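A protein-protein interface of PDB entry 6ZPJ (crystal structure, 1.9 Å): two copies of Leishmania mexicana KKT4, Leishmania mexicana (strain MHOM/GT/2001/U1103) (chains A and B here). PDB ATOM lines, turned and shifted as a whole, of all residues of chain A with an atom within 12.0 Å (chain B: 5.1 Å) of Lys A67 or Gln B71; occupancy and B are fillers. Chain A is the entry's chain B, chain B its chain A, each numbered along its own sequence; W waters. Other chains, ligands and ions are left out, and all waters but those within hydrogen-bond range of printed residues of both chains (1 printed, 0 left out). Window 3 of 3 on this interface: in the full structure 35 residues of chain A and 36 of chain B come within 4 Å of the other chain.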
ATOM      1  N   HIS A  58     -23.247  -3.157 -30.485  1.00  0.00           N
ATOM      2  CA  HIS A  58     -22.370  -4.344 -30.408  1.00  0.00           C
ATOM      3  C   HIS A  58     -21.127  -4.079 -31.257  1.00  0.00           C
ATOM      4  O   HIS A  58     -20.053  -4.493 -30.865  1.00  0.00           O
ATOM      5  CB  HIS A  58     -23.120  -5.601 -30.842  1.00  0.00           C
ATOM      6  CG  HIS A  58     -24.176  -6.029 -29.885  1.00  0.00           C
ATOM      7  ND1 HIS A  58     -25.199  -6.870 -30.253  1.00  0.00           N
ATOM      8  CD2 HIS A  58     -24.387  -5.723 -28.591  1.00  0.00           C
ATOM      9  CE1 HIS A  58     -25.984  -7.078 -29.219  1.00  0.00           C
ATOM     10  NE2 HIS A  58     -25.513  -6.382 -28.191  1.00  0.00           N
ATOM     11  N   ALA A  59     -21.310  -3.457 -32.407  1.00  0.00           N
ATOM     12  CA  ALA A  59     -20.179  -3.160 -33.297  1.00  0.00           C
ATOM     13  C   ALA A  59     -19.260  -2.141 -32.626  1.00  0.00           C
ATOM     14  O   ALA A  59     -18.064  -2.346 -32.647  1.00  0.00           O
ATOM     15  CB  ALA A  59     -20.713  -2.634 -34.590  1.00  0.00           C
ATOM     16  N   TYR A  60     -19.817  -1.096 -32.058  1.00  0.00           N
ATOM     17  CA  TYR A  60     -19.003  -0.097 -31.350  1.00  0.00           C
ATOM     18  C   TYR A  60     -18.210  -0.803 -30.243  1.00  0.00           C
ATOM     19  O   TYR A  60     -17.011  -0.629 -30.167  1.00  0.00           O
ATOM     20  CB  TYR A  60     -19.872   0.993 -30.749  1.00  0.00           C
ATOM     21  CG  TYR A  60     -19.215   1.824 -29.685  1.00  0.00           C
ATOM     22  CD1 TYR A  60     -18.328   2.831 -30.014  1.00  0.00           C
ATOM     23  CD2 TYR A  60     -19.487   1.608 -28.350  1.00  0.00           C
ATOM     24  CE1 TYR A  60     -17.732   3.605 -29.037  1.00  0.00           C
ATOM     25  CE2 TYR A  60     -18.893   2.364 -27.360  1.00  0.00           C
ATOM     26  CZ  TYR A  60     -18.001   3.361 -27.704  1.00  0.00           C
ATOM     27  OH  TYR A  60     -17.433   4.107 -26.719  1.00  0.00           O
ATOM     28  N   ASN A  61     -18.899  -1.576 -29.410  1.00  0.00           N
ATOM     29  CA  ASN A  61     -18.225  -2.248 -28.265  1.00  0.00           C
ATOM     30  C   ASN A  61     -17.115  -3.169 -28.798  1.00  0.00           C
ATOM     31  O   ASN A  61     -16.061  -3.202 -28.198  1.00  0.00           O
ATOM     32  CB  ASN A  61     -19.253  -2.900 -27.325  1.00  0.00           C
ATOM     33  CG  ASN A  61     -20.045  -1.938 -26.477  1.00  0.00           C
ATOM     34  OD1 ASN A  61     -19.585  -0.858 -26.153  1.00  0.00           O
ATOM     35  ND2 ASN A  61     -21.245  -2.339 -26.103  1.00  0.00           N
ATOM     36  N   ALA A  62     -17.342  -3.866 -29.895  1.00  0.00           N
ATOM     37  CA  ALA A  62     -16.338  -4.791 -30.443  1.00  0.00           C
ATOM     38  C   ALA A  62     -15.120  -3.997 -30.927  1.00  0.00           C
ATOM     39  O   ALA A  62     -14.003  -4.447 -30.725  1.00  0.00           O
ATOM     40  CB  ALA A  62     -16.896  -5.607 -31.553  1.00  0.00           C
ATOM     41  N   VAL A  63     -15.374  -2.867 -31.567  1.00  0.00           N
ATOM     42  CA  VAL A  63     -14.279  -2.046 -32.067  1.00  0.00           C
ATOM     43  C   VAL A  63     -13.461  -1.491 -30.910  1.00  0.00           C
ATOM     44  O   VAL A  63     -12.223  -1.468 -30.965  1.00  0.00           O
ATOM     45  CB  VAL A  63     -14.831  -0.932 -32.980  1.00  0.00           C
ATOM     46  CG1 VAL A  63     -13.712   0.051 -33.405  1.00  0.00           C
ATOM     47  CG2 VAL A  63     -15.475  -1.537 -34.201  1.00  0.00           C
ATOM     48  N   ILE A  64     -14.120  -1.024 -29.851  1.00  0.00           N
ATOM     49  CA  ILE A  64     -13.371  -0.521 -28.705  1.00  0.00           C
ATOM     50  C   ILE A  64     -12.527  -1.640 -28.104  1.00  0.00           C
ATOM     51  O   ILE A  64     -11.338  -1.460 -27.823  1.00  0.00           O
ATOM     52  CB  ILE A  64     -14.316   0.098 -27.665  1.00  0.00           C
ATOM     53  CG1 ILE A  64     -15.052   1.293 -28.276  1.00  0.00           C
ATOM     54  CG2 ILE A  64     -13.540   0.492 -26.417  1.00  0.00           C
ATOM     55  CD1 ILE A  64     -14.139   2.450 -28.586  1.00  0.00           C
ATOM     56  N   HIS A  65     -13.127  -2.823 -27.932  1.00  0.00           N
ATOM     57  CA  HIS A  65     -12.383  -3.970 -27.414  1.00  0.00           C
ATOM     58  C   HIS A  65     -11.184  -4.307 -28.308  1.00  0.00           C
ATOM     59  O   HIS A  65     -10.060  -4.487 -27.818  1.00  0.00           O
ATOM     60  CB  HIS A  65     -13.334  -5.173 -27.261  1.00  0.00           C
ATOM     61  CG  HIS A  65     -12.641  -6.432 -26.846  1.00  0.00           C
ATOM     62  ND1 HIS A  65     -12.152  -7.349 -27.753  1.00  0.00           N
ATOM     63  CD2 HIS A  65     -12.329  -6.912 -25.621  1.00  0.00           C
ATOM     64  CE1 HIS A  65     -11.571  -8.341 -27.103  1.00  0.00           C
ATOM     65  NE2 HIS A  65     -11.661  -8.098 -25.808  1.00  0.00           N
ATOM     66  N   ARG A  66     -11.402  -4.383 -29.627  1.00  0.00           N
ATOM     67  CA  ARG A  66     -10.322  -4.719 -30.556  1.00  0.00           C
ATOM     68  C   ARG A  66      -9.179  -3.711 -30.481  1.00  0.00           C
ATOM     69  O   ARG A  66      -8.003  -4.092 -30.445  1.00  0.00           O
ATOM     70  CB  ARG A  66     -10.864  -4.794 -31.981  1.00  0.00           C
ATOM     71  N   LYS A  67      -9.502  -2.414 -30.468  1.00  0.00           N
ATOM     72  CA  LYS A  67      -8.451  -1.399 -30.445  1.00  0.00           C
ATOM     73  C   LYS A  67      -7.698  -1.374 -29.121  1.00  0.00           C
ATOM     74  O   LYS A  67      -6.520  -1.000 -29.092  1.00  0.00           O
ATOM     75  CB  LYS A  67      -9.041  -0.028 -30.747  1.00  0.00           C
ATOM     76  CG  LYS A  67      -9.473   0.079 -32.182  1.00  0.00           C
ATOM     77  CD  LYS A  67     -10.044   1.436 -32.506  1.00  0.00           C
ATOM     78  CE  LYS A  67     -10.257   1.564 -34.007  1.00  0.00           C
ATOM     79  NZ  LYS A  67      -8.980   1.340 -34.761  1.00  0.00           N
ATOM     80  N   ASP A  68      -8.363  -1.740 -28.021  1.00  0.00           N
ATOM     81  CA  ASP A  68      -7.668  -1.916 -26.750  1.00  0.00           C
ATOM     82  C   ASP A  68      -6.660  -3.059 -26.842  1.00  0.00           C
ATOM     83  O   ASP A  68      -5.492  -2.914 -26.447  1.00  0.00           O
ATOM     84  CB  ASP A  68      -8.679  -2.166 -25.621  1.00  0.00           C
ATOM     85  CG  ASP A  68      -9.308  -0.878 -25.094  1.00  0.00           C
ATOM     86  OD1 ASP A  68      -8.643   0.182 -25.141  1.00  0.00           O
ATOM     87  OD2 ASP A  68     -10.473  -0.921 -24.636  1.00  0.00           O
ATOM     88  N   GLU A  69      -7.092  -4.201 -27.391  1.00  0.00           N
ATOM     89  CA  GLU A  69      -6.199  -5.352 -27.511  1.00  0.00           C
ATOM     90  C   GLU A  69      -4.969  -5.017 -28.356  1.00  0.00           C
ATOM     91  O   GLU A  69      -3.826  -5.239 -27.931  1.00  0.00           O
ATOM     92  CB  GLU A  69      -6.964  -6.541 -28.100  1.00  0.00           C
ATOM     93  CG  GLU A  69      -8.049  -7.079 -27.182  1.00  0.00           C
ATOM     94  CD  GLU A  69      -7.492  -7.571 -25.844  1.00  0.00           C
ATOM     95  OE1 GLU A  69      -6.509  -8.346 -25.854  1.00  0.00           O
ATOM     96  OE2 GLU A  69      -8.029  -7.178 -24.782  1.00  0.00           O
ATOM     97  N   VAL A  70      -5.191  -4.483 -29.563  1.00  0.00           N
ATOM     98  CA  VAL A  70      -4.085  -4.120 -30.449  1.00  0.00           C
ATOM     99  C   VAL A  70      -3.107  -3.189 -29.737  1.00  0.00           C
ATOM    100  O   VAL A  70      -1.894  -3.428 -29.715  1.00  0.00           O
ATOM    101  CB  VAL A  70      -4.628  -3.486 -31.741  1.00  0.00           C
ATOM    102  CG1 VAL A  70      -3.487  -2.992 -32.607  1.00  0.00           C
ATOM    103  CG2 VAL A  70      -5.490  -4.487 -32.494  1.00  0.00           C
ATOM    104  N   GLN A  71      -3.607  -2.107 -29.173  1.00  0.00           N
ATOM    105  CA  GLN A  71      -2.764  -1.157 -28.426  1.00  0.00           C
ATOM    106  C   GLN A  71      -1.984  -1.911 -27.345  1.00  0.00           C
ATOM    107  O   GLN A  71      -0.777  -1.735 -27.261  1.00  0.00           O
ATOM    108  CB  GLN A  71      -3.607  -0.034 -27.834  1.00  0.00           C
ATOM    109  CG  GLN A  71      -2.816   1.144 -27.285  1.00  0.00           C
ATOM    110  CD  GLN A  71      -2.123   2.071 -28.271  1.00  0.00           C
ATOM    111  OE1 GLN A  71      -2.015   1.812 -29.460  1.00  0.00           O
ATOM    112  NE2 GLN A  71      -1.618   3.168 -27.757  1.00  0.00           N
ATOM    113  N   GLU A  72      -2.664  -2.768 -26.601  1.00  0.00           N
ATOM    114  CA  GLU A  72      -1.992  -3.542 -25.559  1.00  0.00           C
ATOM    115  C   GLU A  72      -0.823  -4.332 -26.142  1.00  0.00           C
ATOM    116  O   GLU A  72       0.300  -4.282 -25.622  1.00  0.00           O
ATOM    117  CB  GLU A  72      -3.008  -4.465 -24.868  1.00  0.00           C
ATOM    118  N   GLU A  73      -1.064  -5.056 -27.241  1.00  0.00           N
ATOM    119  CA  GLU A  73       0.004  -5.841 -27.860  1.00  0.00           C
ATOM    120  C   GLU A  73       1.139  -4.945 -28.347  1.00  0.00           C
ATOM    121  O   GLU A  73       2.321  -5.304 -28.240  1.00  0.00           O
ATOM    122  CB  GLU A  73      -0.561  -6.675 -29.009  1.00  0.00           C
ATOM    123  N   ALA A  74       0.803  -3.770 -28.879  1.00  0.00           N
ATOM    124  CA  ALA A  74       1.841  -2.833 -29.299  1.00  0.00           C
ATOM    125  C   ALA A  74       2.714  -2.407 -28.119  1.00  0.00           C
ATOM    126  O   ALA A  74       3.947  -2.360 -28.234  1.00  0.00           O
ATOM    127  CB  ALA A  74       1.201  -1.619 -29.978  1.00  0.00           C
ATOM    128  N   LEU A  75       2.096  -2.103 -26.975  1.00  0.00           N
ATOM    129  CA  LEU A  75       2.850  -1.616 -25.824  1.00  0.00           C
ATOM    130  C   LEU A  75       3.617  -2.731 -25.122  1.00  0.00           C
ATOM    131  O   LEU A  75       4.690  -2.480 -24.558  1.00  0.00           O
ATOM    132  CB  LEU A  75       1.912  -0.915 -24.839  1.00  0.00           C
ATOM    133  N   ARG A  76       3.093  -3.960 -25.135  1.00  0.00           N
ATOM    134  CA  ARG A  76       3.873  -5.082 -24.620  1.00  0.00           C
ATOM    135  C   ARG A  76       5.097  -5.341 -25.500  1.00  0.00           C
ATOM    136  O   ARG A  76       6.192  -5.611 -24.991  1.00  0.00           O
ATOM    137  CB  ARG A  76       2.992  -6.333 -24.499  1.00  0.00           C
ATOM    138  N   ILE B  64     -14.682   6.490 -31.420  1.00  0.00           N
ATOM    139  CA  ILE B  64     -13.702   5.607 -32.048  1.00  0.00           C
ATOM    140  C   ILE B  64     -12.558   6.425 -32.645  1.00  0.00           C
ATOM    141  O   ILE B  64     -11.373   6.083 -32.501  1.00  0.00           O
ATOM    142  CB  ILE B  64     -14.390   4.725 -33.105  1.00  0.00           C
ATOM    143  CG1 ILE B  64     -15.367   3.750 -32.431  1.00  0.00           C
ATOM    144  CG2 ILE B  64     -13.363   4.006 -33.976  1.00  0.00           C
ATOM    145  CD1 ILE B  64     -16.366   3.154 -33.366  1.00  0.00           C
ATOM    146  N   ARG B  66     -11.482   9.423 -31.775  1.00  0.00           N
ATOM    147  CA  ARG B  66     -10.648   9.987 -30.737  1.00  0.00           C
ATOM    148  C   ARG B  66      -9.751   8.914 -30.137  1.00  0.00           C
ATOM    149  O   ARG B  66      -8.569   9.159 -29.828  1.00  0.00           O
ATOM    150  CB  ARG B  66     -11.535  10.621 -29.669  1.00  0.00           C
ATOM    151  CG  ARG B  66     -10.781  10.985 -28.393  1.00  0.00           C
ATOM    152  CD  ARG B  66     -11.714  11.502 -27.308  1.00  0.00           C
ATOM    153  NE  ARG B  66     -12.414  10.396 -26.653  1.00  0.00           N
ATOM    154  CZ  ARG B  66     -13.179  10.533 -25.577  1.00  0.00           C
ATOM    155  NH1 ARG B  66     -13.343  11.734 -25.040  1.00  0.00           N
ATOM    156  NH2 ARG B  66     -13.763   9.472 -25.029  1.00  0.00           N
ATOM    157  N   LYS B  67     -10.279   7.699 -30.009  1.00  0.00           N
ATOM    158  CA  LYS B  67      -9.463   6.605 -29.491  1.00  0.00           C
ATOM    159  C   LYS B  67      -8.283   6.314 -30.407  1.00  0.00           C
ATOM    160  O   LYS B  67      -7.153   6.130 -29.937  1.00  0.00           O
ATOM    161  CB  LYS B  67     -10.320   5.352 -29.303  1.00  0.00           C
ATOM    162  CG  LYS B  67      -9.575   4.200 -28.589  1.00  0.00           C
ATOM    163  CD  LYS B  67     -10.526   3.038 -28.321  1.00  0.00           C
ATOM    164  CE  LYS B  67      -9.830   1.953 -27.535  1.00  0.00           C
ATOM    165  NZ  LYS B  67      -9.471   2.449 -26.176  1.00  0.00           N
ATOM    166  N   ASP B  68      -8.520   6.267 -31.720  1.00  0.00           N
ATOM    167  CA  ASP B  68      -7.411   6.079 -32.652  1.00  0.00           C
ATOM    168  C   ASP B  68      -6.404   7.214 -32.529  1.00  0.00           C
ATOM    169  O   ASP B  68      -5.195   6.978 -32.413  1.00  0.00           O
ATOM    170  CB  ASP B  68      -7.929   5.985 -34.088  1.00  0.00           C
ATOM    171  CG  ASP B  68      -8.487   4.612 -34.430  1.00  0.00           C
ATOM    172  OD1 ASP B  68      -8.126   3.614 -33.754  1.00  0.00           O
ATOM    173  OD2 ASP B  68      -9.292   4.529 -35.387  1.00  0.00           O
ATOM    174  N   GLU B  69      -6.894   8.443 -32.482  1.00  0.00           N
ATOM    175  CA  GLU B  69      -6.001   9.623 -32.409  1.00  0.00           C
ATOM    176  C   GLU B  69      -5.134   9.546 -31.149  1.00  0.00           C
ATOM    177  O   GLU B  69      -3.925   9.714 -31.257  1.00  0.00           O
ATOM    178  CB  GLU B  69      -6.851  10.887 -32.397  1.00  0.00           C
ATOM    179  CG  GLU B  69      -6.102  12.183 -32.582  1.00  0.00           C
ATOM    180  CD  GLU B  69      -7.019  13.394 -32.570  1.00  0.00           C
ATOM    181  OE1 GLU B  69      -7.028  14.113 -31.563  1.00  0.00           O
ATOM    182  OE2 GLU B  69      -7.722  13.609 -33.567  1.00  0.00           O
ATOM    183  N   VAL B  70      -5.755   9.307 -30.008  1.00  0.00           N
ATOM    184  CA  VAL B  70      -5.025   9.298 -28.712  1.00  0.00           C
ATOM    185  C   VAL B  70      -4.048   8.121 -28.647  1.00  0.00           C
ATOM    186  O   VAL B  70      -2.929   8.300 -28.201  1.00  0.00           O
ATOM    187  CB  VAL B  70      -6.031   9.317 -27.547  1.00  0.00           C
ATOM    188  CG1 VAL B  70      -5.428   8.856 -26.233  1.00  0.00           C
ATOM    189  CG2 VAL B  70      -6.680  10.679 -27.393  1.00  0.00           C
ATOM    190  N   GLN B  71      -4.459   6.983 -29.142  1.00  0.00           N
ATOM    191  CA  GLN B  71      -3.591   5.805 -29.105  1.00  0.00           C
ATOM    192  C   GLN B  71      -2.398   6.041 -30.017  1.00  0.00           C
ATOM    193  O   GLN B  71      -1.307   5.686 -29.620  1.00  0.00           O
ATOM    194  CB  GLN B  71      -4.383   4.557 -29.479  1.00  0.00           C
ATOM    195  CG  GLN B  71      -5.280   4.090 -28.342  1.00  0.00           C
ATOM    196  CD  GLN B  71      -5.950   2.765 -28.603  1.00  0.00           C
ATOM    197  OE1 GLN B  71      -6.104   2.335 -29.739  1.00  0.00           O
ATOM    198  NE2 GLN B  71      -6.330   2.096 -27.530  1.00  0.00           N
ATOM    199  N   GLU B  72      -2.654   6.531 -31.228  1.00  0.00           N
ATOM    200  CA  GLU B  72      -1.557   6.734 -32.175  1.00  0.00           C
ATOM    201  C   GLU B  72      -0.558   7.761 -31.657  1.00  0.00           C
ATOM    202  O   GLU B  72       0.659   7.602 -31.826  1.00  0.00           O
ATOM    203  CB  GLU B  72      -2.115   7.142 -33.535  1.00  0.00           C
ATOM    204  CG  GLU B  72      -1.050   7.179 -34.629  1.00  0.00           C
ATOM    205  CD  GLU B  72      -1.572   7.706 -35.948  1.00  0.00           C
ATOM    206  OE1 GLU B  72      -1.182   8.831 -36.314  1.00  0.00           O
ATOM    207  OE2 GLU B  72      -2.369   7.009 -36.618  1.00  0.00           O
ATOM    208  N   GLU B  73      -1.044   8.818 -31.011  1.00  0.00           N
ATOM    209  CA  GLU B  73      -0.115   9.809 -30.478  1.00  0.00           C
ATOM    210  C   GLU B  73       0.670   9.255 -29.288  1.00  0.00           C
ATOM    211  O   GLU B  73       1.839   9.613 -29.096  1.00  0.00           O
ATOM    212  CB  GLU B  73      -0.878  11.086 -30.105  1.00  0.00           C
ATOM    213  CG  GLU B  73      -0.012  12.203 -29.536  1.00  0.00           C
ATOM    214  CD  GLU B  73       0.986  12.773 -30.548  1.00  0.00           C
ATOM    215  OE1 GLU B  73       1.792  13.643 -30.156  1.00  0.00           O
ATOM    216  OE2 GLU B  73       0.960  12.362 -31.735  1.00  0.00           O
ATOM    217  N   ALA B  74       0.056   8.373 -28.491  1.00  0.00           N
ATOM    218  CA  ALA B  74       0.790   7.705 -27.422  1.00  0.00           C
ATOM    219  C   ALA B  74       1.965   6.910 -27.978  1.00  0.00           C
ATOM    220  O   ALA B  74       3.077   7.001 -27.464  1.00  0.00           O
ATOM    221  CB  ALA B  74      -0.142   6.795 -26.622  1.00  0.00           C
ATOM    222  N   LEU B  75       1.743   6.127 -29.041  1.00  0.00           N
ATOM    223  CA  LEU B  75       2.866   5.411 -29.644  1.00  0.00           C
ATOM    224  C   LEU B  75       3.890   6.377 -30.219  1.00  0.00           C
ATOM    225  O   LEU B  75       5.097   6.174 -30.062  1.00  0.00           O
ATOM    226  CB  LEU B  75       2.382   4.453 -30.735  1.00  0.00           C
ATOM    227  CG  LEU B  75       1.398   3.377 -30.260  1.00  0.00           C
ATOM    228  CD1 LEU B  75       1.097   2.364 -31.351  1.00  0.00           C
ATOM    229  CD2 LEU B  75       1.947   2.684 -29.024  1.00  0.00           C
HETATM  230  O   HOH W   1      -5.385   0.046 -31.669  1.00  0.00           O
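OD1 of Asp A68 is in salt-bridge range of NZ of Lys B67 (2.6 Å).
The side-chain carboxylate (OD1) of Asp B68 is in salt-bridge range of the side-chain amino group (NZ) of Lys A67.
OE1 of Gln B71 sits close to O of Lys A67.
NE2 of Gln A71 is in hydrogen-bond range of O of Gln B71 (3.1 Å).
The side-chain amino group (NZ) of Lys B67 sits close to the side-chain amide nitrogen (NE2) of Gln B71, 3.4 Å away.
CD1 of Tyr A60 touches CD1 of Ile B64, at 3.9 Å.
CD of Lys B67 touches CD1 of Ile A64 (3.7 Å).
CG2 of Ile B64 touches CE of Lys A67, 3.95 Å away.
Lys B67 touches Lys A67.
Gln B71 touches Asp A68.
Gln A71 touches Leu B75.
Printed residues of chain B within 4 Å of Tyr A60: Ile B64 (3.9 Å).
Of the printed residues of chain B, Ile A64 touches Lys B67 (3.7 Å).
Of chain B, only Ile B64, Lys B67, Asp B68 and Gln B71 come within 4 Å of Lys A67.
Printed residues of chain B within 4 Å of Asp A68: Lys B67 and Gln B71.
Of the printed residues of chain B, Gln A71 touches Gln B71 (3.1 Å) and Leu B75 (3.7 Å).
Of the printed residues of chain A, Ile B64 touches Tyr A60 (3.9 Å) and Lys A67 (3.95 Å).
Of chain A, only Ile A64 (3.7 Å), Lys A67 (3.9 Å) and Asp A68 (2.6 Å) come within 4 Å of Lys B67.
Of chain A, only Lys A67 comes within 4 Å of Asp B68.
Val B70 touches none of the printed residues of chain A.
Of chain A, only Lys A67 (3.4 Å), Asp A68 (3.8 Å) and Gln A71 (3.1 Å) come within 4 Å of Gln B71.
No residue of chain A comes within 4 Å of Glu B72.
Of the printed residues of chain A, Leu B75 touches Gln A71.
The nearest printed residue of chain B that does not touch Lys A67 is Glu B69 (7.7 Å).
The nearest printed residue of chain A that does not touch Gln B71 is Ile A64 (6.1 Å).
The nearest printed residue of chain B that does not touch Gln A71 is Ala B74 (4.1 Å).
Hydrophobic or aromatic side chains of chain B within 4 Å of the printed part of chain A: Ile B64 and Leu B75.
Of the 19 printed residues of chain A, 5 touch a printed residue of chain B.
Printed residues of chain A that touch a printed residue of chain B: Tyr A60, Ile A64, Lys A67, Asp A68 and Gln A71.
Along chain A the printed residues that touch a printed residue of chain B span positions 60 to 71.
Lys A67 touches Asp B68, and with the chains exchanged Asp A68 touches Lys B67.
Lys A67 touches Gln B71, but with the chains exchanged Gln A71 does not touch Lys B67 (6.5 Å).
Asp A68 touches Gln B71, but with the chains exchanged Gln A71 does not touch Asp B68 (6.7 Å).
Gln B71 touches its own counterpart, Gln A71.
11 positions are printed for both chains.
Of the 10 pairs that touch across the chains among the printed residues, 6 have their exchanged pair printed and touching as well.
Water W1 lies within hydrogen-bond range of O of Lys A67 (3.0 Å) and OE1 of Gln B71 (3.1 Å).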
